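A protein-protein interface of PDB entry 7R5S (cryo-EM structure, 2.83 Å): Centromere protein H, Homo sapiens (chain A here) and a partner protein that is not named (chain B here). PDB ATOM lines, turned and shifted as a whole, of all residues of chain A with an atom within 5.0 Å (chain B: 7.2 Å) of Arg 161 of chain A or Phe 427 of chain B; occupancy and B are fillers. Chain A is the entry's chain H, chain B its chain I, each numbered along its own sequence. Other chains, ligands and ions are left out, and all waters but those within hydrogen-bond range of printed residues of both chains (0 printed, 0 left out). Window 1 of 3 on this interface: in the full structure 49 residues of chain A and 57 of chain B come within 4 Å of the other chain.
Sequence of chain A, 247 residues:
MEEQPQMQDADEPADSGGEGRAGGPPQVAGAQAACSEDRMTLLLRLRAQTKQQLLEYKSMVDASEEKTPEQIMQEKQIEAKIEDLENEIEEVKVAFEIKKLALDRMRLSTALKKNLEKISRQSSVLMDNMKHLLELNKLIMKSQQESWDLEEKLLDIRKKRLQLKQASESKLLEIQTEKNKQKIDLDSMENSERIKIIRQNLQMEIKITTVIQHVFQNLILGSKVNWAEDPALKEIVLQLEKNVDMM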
ATOM      1  N   ASP A 156      22.907   6.583  -1.737  1.00  0.00           N
ATOM      2  CA  ASP A 156      24.251   6.020  -1.820  1.00  0.00           C
ATOM      3  C   ASP A 156      25.031   6.608  -2.989  1.00  0.00           C
ATOM      4  O   ASP A 156      26.243   6.849  -2.873  1.00  0.00           O
ATOM      5  CB  ASP A 156      24.182   4.497  -1.934  1.00  0.00           C
ATOM      6  CG  ASP A 156      23.378   3.864  -0.818  1.00  0.00           C
ATOM      7  OD1 ASP A 156      23.924   3.704   0.293  1.00  0.00           O
ATOM      8  OD2 ASP A 156      22.200   3.522  -1.051  1.00  0.00           O
ATOM      9  N   ILE A 157      24.363   6.842  -4.124  1.00  0.00           N
ATOM     10  CA  ILE A 157      25.068   7.437  -5.261  1.00  0.00           C
ATOM     11  C   ILE A 157      25.649   8.797  -4.877  1.00  0.00           C
ATOM     12  O   ILE A 157      26.833   9.084  -5.115  1.00  0.00           O
ATOM     13  CB  ILE A 157      24.137   7.540  -6.483  1.00  0.00           C
ATOM     14  CG1 ILE A 157      23.915   6.157  -7.094  1.00  0.00           C
ATOM     15  CG2 ILE A 157      24.719   8.493  -7.515  1.00  0.00           C
ATOM     16  CD1 ILE A 157      23.244   6.185  -8.447  1.00  0.00           C
ATOM     17  N   ARG A 158      24.825   9.649  -4.258  1.00  0.00           N
ATOM     18  CA  ARG A 158      25.286  10.981  -3.880  1.00  0.00           C
ATOM     19  C   ARG A 158      26.376  10.916  -2.816  1.00  0.00           C
ATOM     20  O   ARG A 158      27.311  11.727  -2.827  1.00  0.00           O
ATOM     21  CB  ARG A 158      24.106  11.824  -3.401  1.00  0.00           C
ATOM     22  CG  ARG A 158      23.135  12.188  -4.510  1.00  0.00           C
ATOM     23  CD  ARG A 158      21.816  12.702  -3.963  1.00  0.00           C
ATOM     24  NE  ARG A 158      20.914  13.112  -5.036  1.00  0.00           N
ATOM     25  CZ  ARG A 158      19.633  13.417  -4.861  1.00  0.00           C
ATOM     26  NH1 ARG A 158      19.095  13.357  -3.650  1.00  0.00           N
ATOM     27  NH2 ARG A 158      18.888  13.780  -5.896  1.00  0.00           N
ATOM     28  N   LYS A 159      26.278   9.957  -1.891  1.00  0.00           N
ATOM     29  CA  LYS A 159      27.311   9.818  -0.866  1.00  0.00           C
ATOM     30  C   LYS A 159      28.661   9.476  -1.490  1.00  0.00           C
ATOM     31  O   LYS A 159      29.695  10.063  -1.133  1.00  0.00           O
ATOM     32  CB  LYS A 159      26.894   8.752   0.147  1.00  0.00           C
ATOM     33  CG  LYS A 159      27.738   8.725   1.408  1.00  0.00           C
ATOM     34  CD  LYS A 159      27.140   7.791   2.446  1.00  0.00           C
ATOM     35  CE  LYS A 159      25.705   8.172   2.769  1.00  0.00           C
ATOM     36  NZ  LYS A 159      25.090   7.243   3.754  1.00  0.00           N
ATOM     37  N   LYS A 160      28.670   8.527  -2.431  1.00  0.00           N
ATOM     38  CA  LYS A 160      29.919   8.175  -3.101  1.00  0.00           C
ATOM     39  C   LYS A 160      30.478   9.358  -3.885  1.00  0.00           C
ATOM     40  O   LYS A 160      31.695   9.601  -3.878  1.00  0.00           O
ATOM     41  CB  LYS A 160      29.704   6.972  -4.019  1.00  0.00           C
ATOM     42  CG  LYS A 160      29.555   5.653  -3.278  1.00  0.00           C
ATOM     43  CD  LYS A 160      29.537   4.473  -4.236  1.00  0.00           C
ATOM     44  CE  LYS A 160      28.326   4.523  -5.151  1.00  0.00           C
ATOM     45  NZ  LYS A 160      28.265   3.341  -6.054  1.00  0.00           N
ATOM     46  N   ARG A 161      29.604  10.106  -4.567  1.00  0.00           N
ATOM     47  CA  ARG A 161      30.062  11.293  -5.287  1.00  0.00           C
ATOM     48  C   ARG A 161      30.722  12.295  -4.346  1.00  0.00           C
ATOM     49  O   ARG A 161      31.779  12.860  -4.664  1.00  0.00           O
ATOM     50  CB  ARG A 161      28.893  11.946  -6.022  1.00  0.00           C
ATOM     51  CG  ARG A 161      28.584  11.342  -7.378  1.00  0.00           C
ATOM     52  CD  ARG A 161      27.643  12.243  -8.152  1.00  0.00           C
ATOM     53  NE  ARG A 161      28.156  13.607  -8.231  1.00  0.00           N
ATOM     54  CZ  ARG A 161      27.398  14.682  -8.420  1.00  0.00           C
ATOM     55  NH1 ARG A 161      26.086  14.556  -8.546  1.00  0.00           N
ATOM     56  NH2 ARG A 161      27.954  15.884  -8.477  1.00  0.00           N
ATOM     57  N   LEU A 162      30.109  12.531  -3.182  1.00  0.00           N
ATOM     58  CA  LEU A 162      30.668  13.493  -2.237  1.00  0.00           C
ATOM     59  C   LEU A 162      32.025  13.035  -1.716  1.00  0.00           C
ATOM     60  O   LEU A 162      32.948  13.846  -1.570  1.00  0.00           O
ATOM     61  CB  LEU A 162      29.694  13.720  -1.080  1.00  0.00           C
ATOM     62  CG  LEU A 162      30.030  14.869  -0.130  1.00  0.00           C
ATOM     63  CD1 LEU A 162      30.342  16.137  -0.908  1.00  0.00           C
ATOM     64  CD2 LEU A 162      28.891  15.106   0.846  1.00  0.00           C
ATOM     65  N   GLN A 163      32.165  11.738  -1.427  1.00  0.00           N
ATOM     66  CA  GLN A 163      33.458  11.226  -0.975  1.00  0.00           C
ATOM     67  C   GLN A 163      34.533  11.429  -2.040  1.00  0.00           C
ATOM     68  O   GLN A 163      35.658  11.860  -1.740  1.00  0.00           O
ATOM     69  CB  GLN A 163      33.340   9.749  -0.603  1.00  0.00           C
ATOM     70  CG  GLN A 163      32.444   9.479   0.594  1.00  0.00           C
ATOM     71  CD  GLN A 163      32.606   8.074   1.136  1.00  0.00           C
ATOM     72  OE1 GLN A 163      31.628   7.344   1.300  1.00  0.00           O
ATOM     73  NE2 GLN A 163      33.844   7.688   1.417  1.00  0.00           N
ATOM     74  N   LEU A 164      34.201  11.118  -3.298  1.00  0.00           N
ATOM     75  CA  LEU A 164      35.165  11.301  -4.379  1.00  0.00           C
ATOM     76  C   LEU A 164      35.582  12.761  -4.511  1.00  0.00           C
ATOM     77  O   LEU A 164      36.769  13.061  -4.702  1.00  0.00           O
ATOM     78  CB  LEU A 164      34.582  10.794  -5.697  1.00  0.00           C
ATOM     79  CG  LEU A 164      34.468   9.279  -5.844  1.00  0.00           C
ATOM     80  CD1 LEU A 164      33.690   8.937  -7.097  1.00  0.00           C
ATOM     81  CD2 LEU A 164      35.847   8.643  -5.877  1.00  0.00           C
ATOM     82  N   LYS A 165      34.619  13.681  -4.422  1.00  0.00           N
ATOM     83  CA  LYS A 165      34.943  15.104  -4.497  1.00  0.00           C
ATOM     84  C   LYS A 165      35.870  15.516  -3.358  1.00  0.00           C
ATOM     85  O   LYS A 165      36.857  16.238  -3.570  1.00  0.00           O
ATOM     86  CB  LYS A 165      33.659  15.933  -4.473  1.00  0.00           C
ATOM     87  CG  LYS A 165      33.883  17.424  -4.280  1.00  0.00           C
ATOM     88  CD  LYS A 165      32.564  18.167  -4.157  1.00  0.00           C
ATOM     89  CE  LYS A 165      32.786  19.651  -3.913  1.00  0.00           C
ATOM     90  NZ  LYS A 165      33.552  19.897  -2.661  1.00  0.00           N
ATOM     91  N   SER B 370      30.922  21.889 -19.121  1.00  0.00           N
ATOM     92  CA  SER B 370      31.073  20.771 -18.195  1.00  0.00           C
ATOM     93  C   SER B 370      32.540  20.480 -17.902  1.00  0.00           C
ATOM     94  O   SER B 370      32.893  20.118 -16.772  1.00  0.00           O
ATOM     95  CB  SER B 370      30.383  19.529 -18.757  1.00  0.00           C
ATOM     96  OG  SER B 370      29.106  19.849 -19.278  1.00  0.00           O
ATOM     97  N   LEU B 373      33.548  22.919 -15.366  1.00  0.00           N
ATOM     98  CA  LEU B 373      32.891  22.609 -14.101  1.00  0.00           C
ATOM     99  C   LEU B 373      33.609  21.476 -13.380  1.00  0.00           C
ATOM    100  O   LEU B 373      33.762  21.510 -12.154  1.00  0.00           O
ATOM    101  CB  LEU B 373      31.425  22.251 -14.339  1.00  0.00           C
ATOM    102  CG  LEU B 373      30.451  23.407 -14.573  1.00  0.00           C
ATOM    103  CD1 LEU B 373      29.066  22.881 -14.908  1.00  0.00           C
ATOM    104  CD2 LEU B 373      30.395  24.315 -13.358  1.00  0.00           C
ATOM    105  N   HIS B 374      34.066  20.468 -14.127  1.00  0.00           N
ATOM    106  CA  HIS B 374      34.819  19.378 -13.516  1.00  0.00           C
ATOM    107  C   HIS B 374      36.117  19.874 -12.892  1.00  0.00           C
ATOM    108  O   HIS B 374      36.587  19.302 -11.902  1.00  0.00           O
ATOM    109  CB  HIS B 374      35.114  18.291 -14.550  1.00  0.00           C
ATOM    110  CG  HIS B 374      34.062  17.229 -14.627  1.00  0.00           C
ATOM    111  ND1 HIS B 374      33.165  17.144 -15.669  1.00  0.00           N
ATOM    112  CD2 HIS B 374      33.764  16.208 -13.789  1.00  0.00           C
ATOM    113  CE1 HIS B 374      32.360  16.116 -15.471  1.00  0.00           C
ATOM    114  NE2 HIS B 374      32.702  15.531 -14.338  1.00  0.00           N
ATOM    115  N   TYR B 375      36.709  20.930 -13.451  1.00  0.00           N
ATOM    116  CA  TYR B 375      37.927  21.487 -12.877  1.00  0.00           C
ATOM    117  C   TYR B 375      37.623  22.325 -11.641  1.00  0.00           C
ATOM    118  O   TYR B 375      38.265  22.162 -10.598  1.00  0.00           O
ATOM    119  CB  TYR B 375      38.671  22.323 -13.919  1.00  0.00           C
ATOM    120  CG  TYR B 375      39.843  23.095 -13.357  1.00  0.00           C
ATOM    121  CD1 TYR B 375      41.049  22.463 -13.084  1.00  0.00           C
ATOM    122  CD2 TYR B 375      39.745  24.456 -13.097  1.00  0.00           C
ATOM    123  CE1 TYR B 375      42.123  23.163 -12.570  1.00  0.00           C
ATOM    124  CE2 TYR B 375      40.814  25.163 -12.581  1.00  0.00           C
ATOM    125  CZ  TYR B 375      41.999  24.513 -12.320  1.00  0.00           C
ATOM    126  OH  TYR B 375      43.067  25.213 -11.808  1.00  0.00           O
ATOM    127  N   ILE B 376      36.644  23.228 -11.739  1.00  0.00           N
ATOM    128  CA  ILE B 376      36.308  24.084 -10.605  1.00  0.00           C
ATOM    129  C   ILE B 376      35.587  23.337  -9.494  1.00  0.00           C
ATOM    130  O   ILE B 376      35.344  23.917  -8.431  1.00  0.00           O
ATOM    131  CB  ILE B 376      35.451  25.291 -11.035  1.00  0.00           C
ATOM    132  CG1 ILE B 376      34.028  24.849 -11.374  1.00  0.00           C
ATOM    133  CG2 ILE B 376      36.095  26.018 -12.207  1.00  0.00           C
ATOM    134  CD1 ILE B 376      33.062  26.000 -11.535  1.00  0.00           C
ATOM    135  N   ASN B 377      35.224  22.070  -9.718  1.00  0.00           N
ATOM    136  CA  ASN B 377      34.633  21.276  -8.646  1.00  0.00           C
ATOM    137  C   ASN B 377      35.590  21.134  -7.471  1.00  0.00           C
ATOM    138  O   ASN B 377      35.170  21.181  -6.310  1.00  0.00           O
ATOM    139  CB  ASN B 377      34.230  19.900  -9.177  1.00  0.00           C
ATOM    140  CG  ASN B 377      33.373  19.126  -8.197  1.00  0.00           C
ATOM    141  OD1 ASN B 377      32.802  19.696  -7.268  1.00  0.00           O
ATOM    142  ND2 ASN B 377      33.277  17.818  -8.400  1.00  0.00           N
ATOM    143  N   ILE B 421      21.564  28.094 -13.285  1.00  0.00           N
ATOM    144  CA  ILE B 421      22.268  28.164 -12.005  1.00  0.00           C
ATOM    145  C   ILE B 421      21.933  26.953 -11.142  1.00  0.00           C
ATOM    146  O   ILE B 421      22.810  26.376 -10.487  1.00  0.00           O
ATOM    147  CB  ILE B 421      21.936  29.483 -11.283  1.00  0.00           C
ATOM    148  CG1 ILE B 421      22.543  30.669 -12.032  1.00  0.00           C
ATOM    149  CG2 ILE B 421      22.435  29.453  -9.848  1.00  0.00           C
ATOM    150  CD1 ILE B 421      22.314  31.994 -11.346  1.00  0.00           C
ATOM    151  N   ILE B 422      20.661  26.547 -11.128  1.00  0.00           N
ATOM    152  CA  ILE B 422      20.252  25.402 -10.321  1.00  0.00           C
ATOM    153  C   ILE B 422      20.867  24.118 -10.862  1.00  0.00           C
ATOM    154  O   ILE B 422      21.325  23.263 -10.094  1.00  0.00           O
ATOM    155  CB  ILE B 422      18.716  25.315 -10.264  1.00  0.00           C
ATOM    156  CG1 ILE B 422      18.147  26.480  -9.454  1.00  0.00           C
ATOM    157  CG2 ILE B 422      18.274  23.990  -9.664  1.00  0.00           C
ATOM    158  CD1 ILE B 422      16.650  26.625  -9.572  1.00  0.00           C
ATOM    159  N   ARG B 423      20.894  23.961 -12.187  1.00  0.00           N
ATOM    160  CA  ARG B 423      21.512  22.778 -12.775  1.00  0.00           C
ATOM    161  C   ARG B 423      23.011  22.743 -12.515  1.00  0.00           C
ATOM    162  O   ARG B 423      23.594  21.660 -12.390  1.00  0.00           O
ATOM    163  CB  ARG B 423      21.229  22.731 -14.277  1.00  0.00           C
ATOM    164  CG  ARG B 423      21.503  21.384 -14.921  1.00  0.00           C
ATOM    165  CD  ARG B 423      21.415  21.459 -16.439  1.00  0.00           C
ATOM    166  NE  ARG B 423      20.149  22.030 -16.894  1.00  0.00           N
ATOM    167  CZ  ARG B 423      20.024  23.236 -17.439  1.00  0.00           C
ATOM    168  NH1 ARG B 423      21.092  24.004 -17.604  1.00  0.00           N
ATOM    169  NH2 ARG B 423      18.833  23.672 -17.823  1.00  0.00           N
ATOM    170  N   ALA B 424      23.652  23.911 -12.429  1.00  0.00           N
ATOM    171  CA  ALA B 424      25.081  23.949 -12.141  1.00  0.00           C
ATOM    172  C   ALA B 424      25.368  23.661 -10.672  1.00  0.00           C
ATOM    173  O   ALA B 424      26.360  22.998 -10.352  1.00  0.00           O
ATOM    174  CB  ALA B 424      25.662  25.304 -12.541  1.00  0.00           C
ATOM    175  N   GLU B 425      24.518  24.150  -9.768  1.00  0.00           N
ATOM    176  CA  GLU B 425      24.730  23.947  -8.341  1.00  0.00           C
ATOM    177  C   GLU B 425      24.224  22.598  -7.848  1.00  0.00           C
ATOM    178  O   GLU B 425      24.565  22.201  -6.729  1.00  0.00           O
ATOM    179  CB  GLU B 425      24.069  25.073  -7.538  1.00  0.00           C
ATOM    180  CG  GLU B 425      22.558  24.995  -7.459  1.00  0.00           C
ATOM    181  CD  GLU B 425      21.970  26.094  -6.597  1.00  0.00           C
ATOM    182  OE1 GLU B 425      22.731  26.991  -6.175  1.00  0.00           O
ATOM    183  OE2 GLU B 425      20.749  26.062  -6.341  1.00  0.00           O
ATOM    184  N   CYS B 426      23.418  21.889  -8.643  1.00  0.00           N
ATOM    185  CA  CYS B 426      23.162  20.483  -8.348  1.00  0.00           C
ATOM    186  C   CYS B 426      24.443  19.674  -8.473  1.00  0.00           C
ATOM    187  O   CYS B 426      24.725  18.804  -7.640  1.00  0.00           O
ATOM    188  CB  CYS B 426      22.080  19.935  -9.276  1.00  0.00           C
ATOM    189  SG  CYS B 426      20.389  20.210  -8.698  1.00  0.00           S
ATOM    190  N   PHE B 427      25.227  19.943  -9.513  1.00  0.00           N
ATOM    191  CA  PHE B 427      26.617  19.527  -9.544  1.00  0.00           C
ATOM    192  C   PHE B 427      27.408  20.332  -8.514  1.00  0.00           C
ATOM    193  O   PHE B 427      26.946  21.357  -8.005  1.00  0.00           O
ATOM    194  CB  PHE B 427      27.196  19.721 -10.947  1.00  0.00           C
ATOM    195  CG  PHE B 427      28.410  18.881 -11.231  1.00  0.00           C
ATOM    196  CD1 PHE B 427      28.288  17.525 -11.484  1.00  0.00           C
ATOM    197  CD2 PHE B 427      29.670  19.452 -11.268  1.00  0.00           C
ATOM    198  CE1 PHE B 427      29.403  16.753 -11.753  1.00  0.00           C
ATOM    199  CE2 PHE B 427      30.787  18.686 -11.537  1.00  0.00           C
ATOM    200  CZ  PHE B 427      30.654  17.335 -11.779  1.00  0.00           C
ATOM    201  N   LEU B 428      28.601  19.831  -8.184  1.00  0.00           N
ATOM    202  CA  LEU B 428      29.500  20.414  -7.186  1.00  0.00           C
ATOM    203  C   LEU B 428      28.960  20.214  -5.775  1.00  0.00           C
ATOM    204  O   LEU B 428      29.667  20.473  -4.796  1.00  0.00           O
ATOM    205  CB  LEU B 428      29.746  21.910  -7.439  1.00  0.00           C
ATOM    206  CG  LEU B 428      29.938  22.454  -8.858  1.00  0.00           C
ATOM    207  CD1 LEU B 428      29.875  23.973  -8.853  1.00  0.00           C
ATOM    208  CD2 LEU B 428      31.245  21.982  -9.451  1.00  0.00           C
ATOM    209  N   GLN B 429      27.718  19.732  -5.667  1.00  0.00           N
ATOM    210  CA  GLN B 429      27.081  19.403  -4.389  1.00  0.00           C
ATOM    211  C   GLN B 429      27.214  20.532  -3.367  1.00  0.00           C
ATOM    212  O   GLN B 429      27.459  20.297  -2.182  1.00  0.00           O
ATOM    213  CB  GLN B 429      27.637  18.094  -3.831  1.00  0.00           C
ATOM    214  CG  GLN B 429      27.196  16.867  -4.612  1.00  0.00           C
ATOM    215  CD  GLN B 429      27.930  15.613  -4.193  1.00  0.00           C
ATOM    216  OE1 GLN B 429      27.329  14.670  -3.680  1.00  0.00           O
ATOM    217  NE2 GLN B 429      29.238  15.593  -4.415  1.00  0.00           N
ATOM    218  N   GLU B 430      27.039  21.768  -3.827  1.00  0.00           N
ATOM    219  CA  GLU B 430      27.092  22.934  -2.951  1.00  0.00           C
ATOM    220  C   GLU B 430      26.528  24.129  -3.708  1.00  0.00           C
ATOM    221  O   GLU B 430      26.296  24.070  -4.918  1.00  0.00           O
ATOM    222  CB  GLU B 430      28.516  23.219  -2.467  1.00  0.00           C
ATOM    223  CG  GLU B 430      29.501  23.538  -3.576  1.00  0.00           C
ATOM    224  CD  GLU B 430      30.899  23.796  -3.053  1.00  0.00           C
ATOM    225  OE1 GLU B 430      31.085  23.779  -1.818  1.00  0.00           O
ATOM    226  OE2 GLU B 430      31.813  24.014  -3.876  1.00  0.00           O
ATOM    227  N   GLY B 431      26.311  25.218  -2.975  1.00  0.00           N
ATOM    228  CA  GLY B 431      25.780  26.434  -3.560  1.00  0.00           C
ATOM    229  C   GLY B 431      26.726  27.613  -3.465  1.00  0.00           C
ATOM    230  O   GLY B 431      27.679  27.590  -2.680  1.00  0.00           O
ATOM    231  N   PHE B 432      26.474  28.649  -4.260  1.00  0.00           N
ATOM    232  CA  PHE B 432      27.322  29.830  -4.260  1.00  0.00           C
ATOM    233  C   PHE B 432      26.860  30.827  -3.199  1.00  0.00           C
ATOM    234  O   PHE B 432      25.717  30.802  -2.736  1.00  0.00           O
ATOM    235  CB  PHE B 432      27.318  30.498  -5.636  1.00  0.00           C
ATOM    236  CG  PHE B 432      27.521  29.544  -6.777  1.00  0.00           C
ATOM    237  CD1 PHE B 432      28.789  29.094  -7.104  1.00  0.00           C
ATOM    238  CD2 PHE B 432      26.445  29.104  -7.529  1.00  0.00           C
ATOM    239  CE1 PHE B 432      28.978  28.218  -8.157  1.00  0.00           C
ATOM    240  CE2 PHE B 432      26.629  28.228  -8.581  1.00  0.00           C
ATOM    241  CZ  PHE B 432      27.897  27.785  -8.895  1.00  0.00           C
ATOM    242  N   TRP B 461      19.607  25.070  -1.290  1.00  0.00           N
ATOM    243  CA  TRP B 461      21.070  25.032  -1.282  1.00  0.00           C
ATOM    244  C   TRP B 461      21.639  26.165  -0.427  1.00  0.00           C
ATOM    245  O   TRP B 461      22.312  27.074  -0.911  1.00  0.00           O
ATOM    246  CB  TRP B 461      21.607  25.092  -2.709  1.00  0.00           C
ATOM    247  CG  TRP B 461      21.411  23.822  -3.478  1.00  0.00           C
ATOM    248  CD1 TRP B 461      20.515  23.602  -4.481  1.00  0.00           C
ATOM    249  CD2 TRP B 461      22.126  22.594  -3.301  1.00  0.00           C
ATOM    250  NE1 TRP B 461      20.629  22.314  -4.944  1.00  0.00           N
ATOM    251  CE2 TRP B 461      21.612  21.674  -4.236  1.00  0.00           C
ATOM    252  CE3 TRP B 461      23.153  22.183  -2.446  1.00  0.00           C
ATOM    253  CZ2 TRP B 461      22.088  20.370  -4.338  1.00  0.00           C
ATOM    254  CZ3 TRP B 461      23.623  20.888  -2.549  1.00  0.00           C
ATOM    255  CH2 TRP B 461      23.091  19.997  -3.487  1.00  0.00           C
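Phe 427 of chain B touches Arg 161 of chain A (CD1 to NH2, 3.4 Å).
Gln 429 of chain B touches Arg 161 of chain A (NE2 to C, 3.6 Å).
Lys 165 of chain A touches Asn 377 of chain B.
Lys 165 of chain A touches Leu 428 of chain B (CE to O, 3.3 Å).
Printed residues of chain B within 4 Å of Arg 161 of chain A: Phe 427 and Gln 429.
Of chain A, only Arg 161 comes within 4 Å of Phe 427 of chain B.
Of the printed residues of chain A, Gln 429 of chain B touches Arg 158 (3.1 Å), Arg 161 (3.6 Å) and Leu 162 (3.3 Å).
Printed residues of chain B within 4 Å of Lys 165 of chain A: Asn 377 (3.4 Å) and Leu 428 (3.3 Å).
Of the printed residues of chain A, Asn 377 of chain B touches Lys 165 (3.4 Å).
Of the printed residues of chain B, Arg 158 of chain A touches Gln 429.
The nearest printed residue of chain A that does not touch Phe 427 of chain B is Lys 165 of chain A (7.1 Å).
The nearest printed residue of chain A that does not touch Asn 377 of chain B is Arg 161 of chain A (5.7 Å).
Hydrophobic or aromatic side chains of chain B within 4 Å of the printed part of chain A: Phe 427.
Of the 10 printed residues of chain A, 4 touch a printed residue of chain B.
Among the printed residues, 6 pairs touch across the chains.
N of Leu 162 of chain A sits close to NE2 of Gln 429 of chain B, at 3.4 Å.
The backbone carbonyl oxygen (O) of Arg 158 of chain A sits close to the side-chain amide oxygen (OE1) of Gln 429 of chain B, 3.1 Å away.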
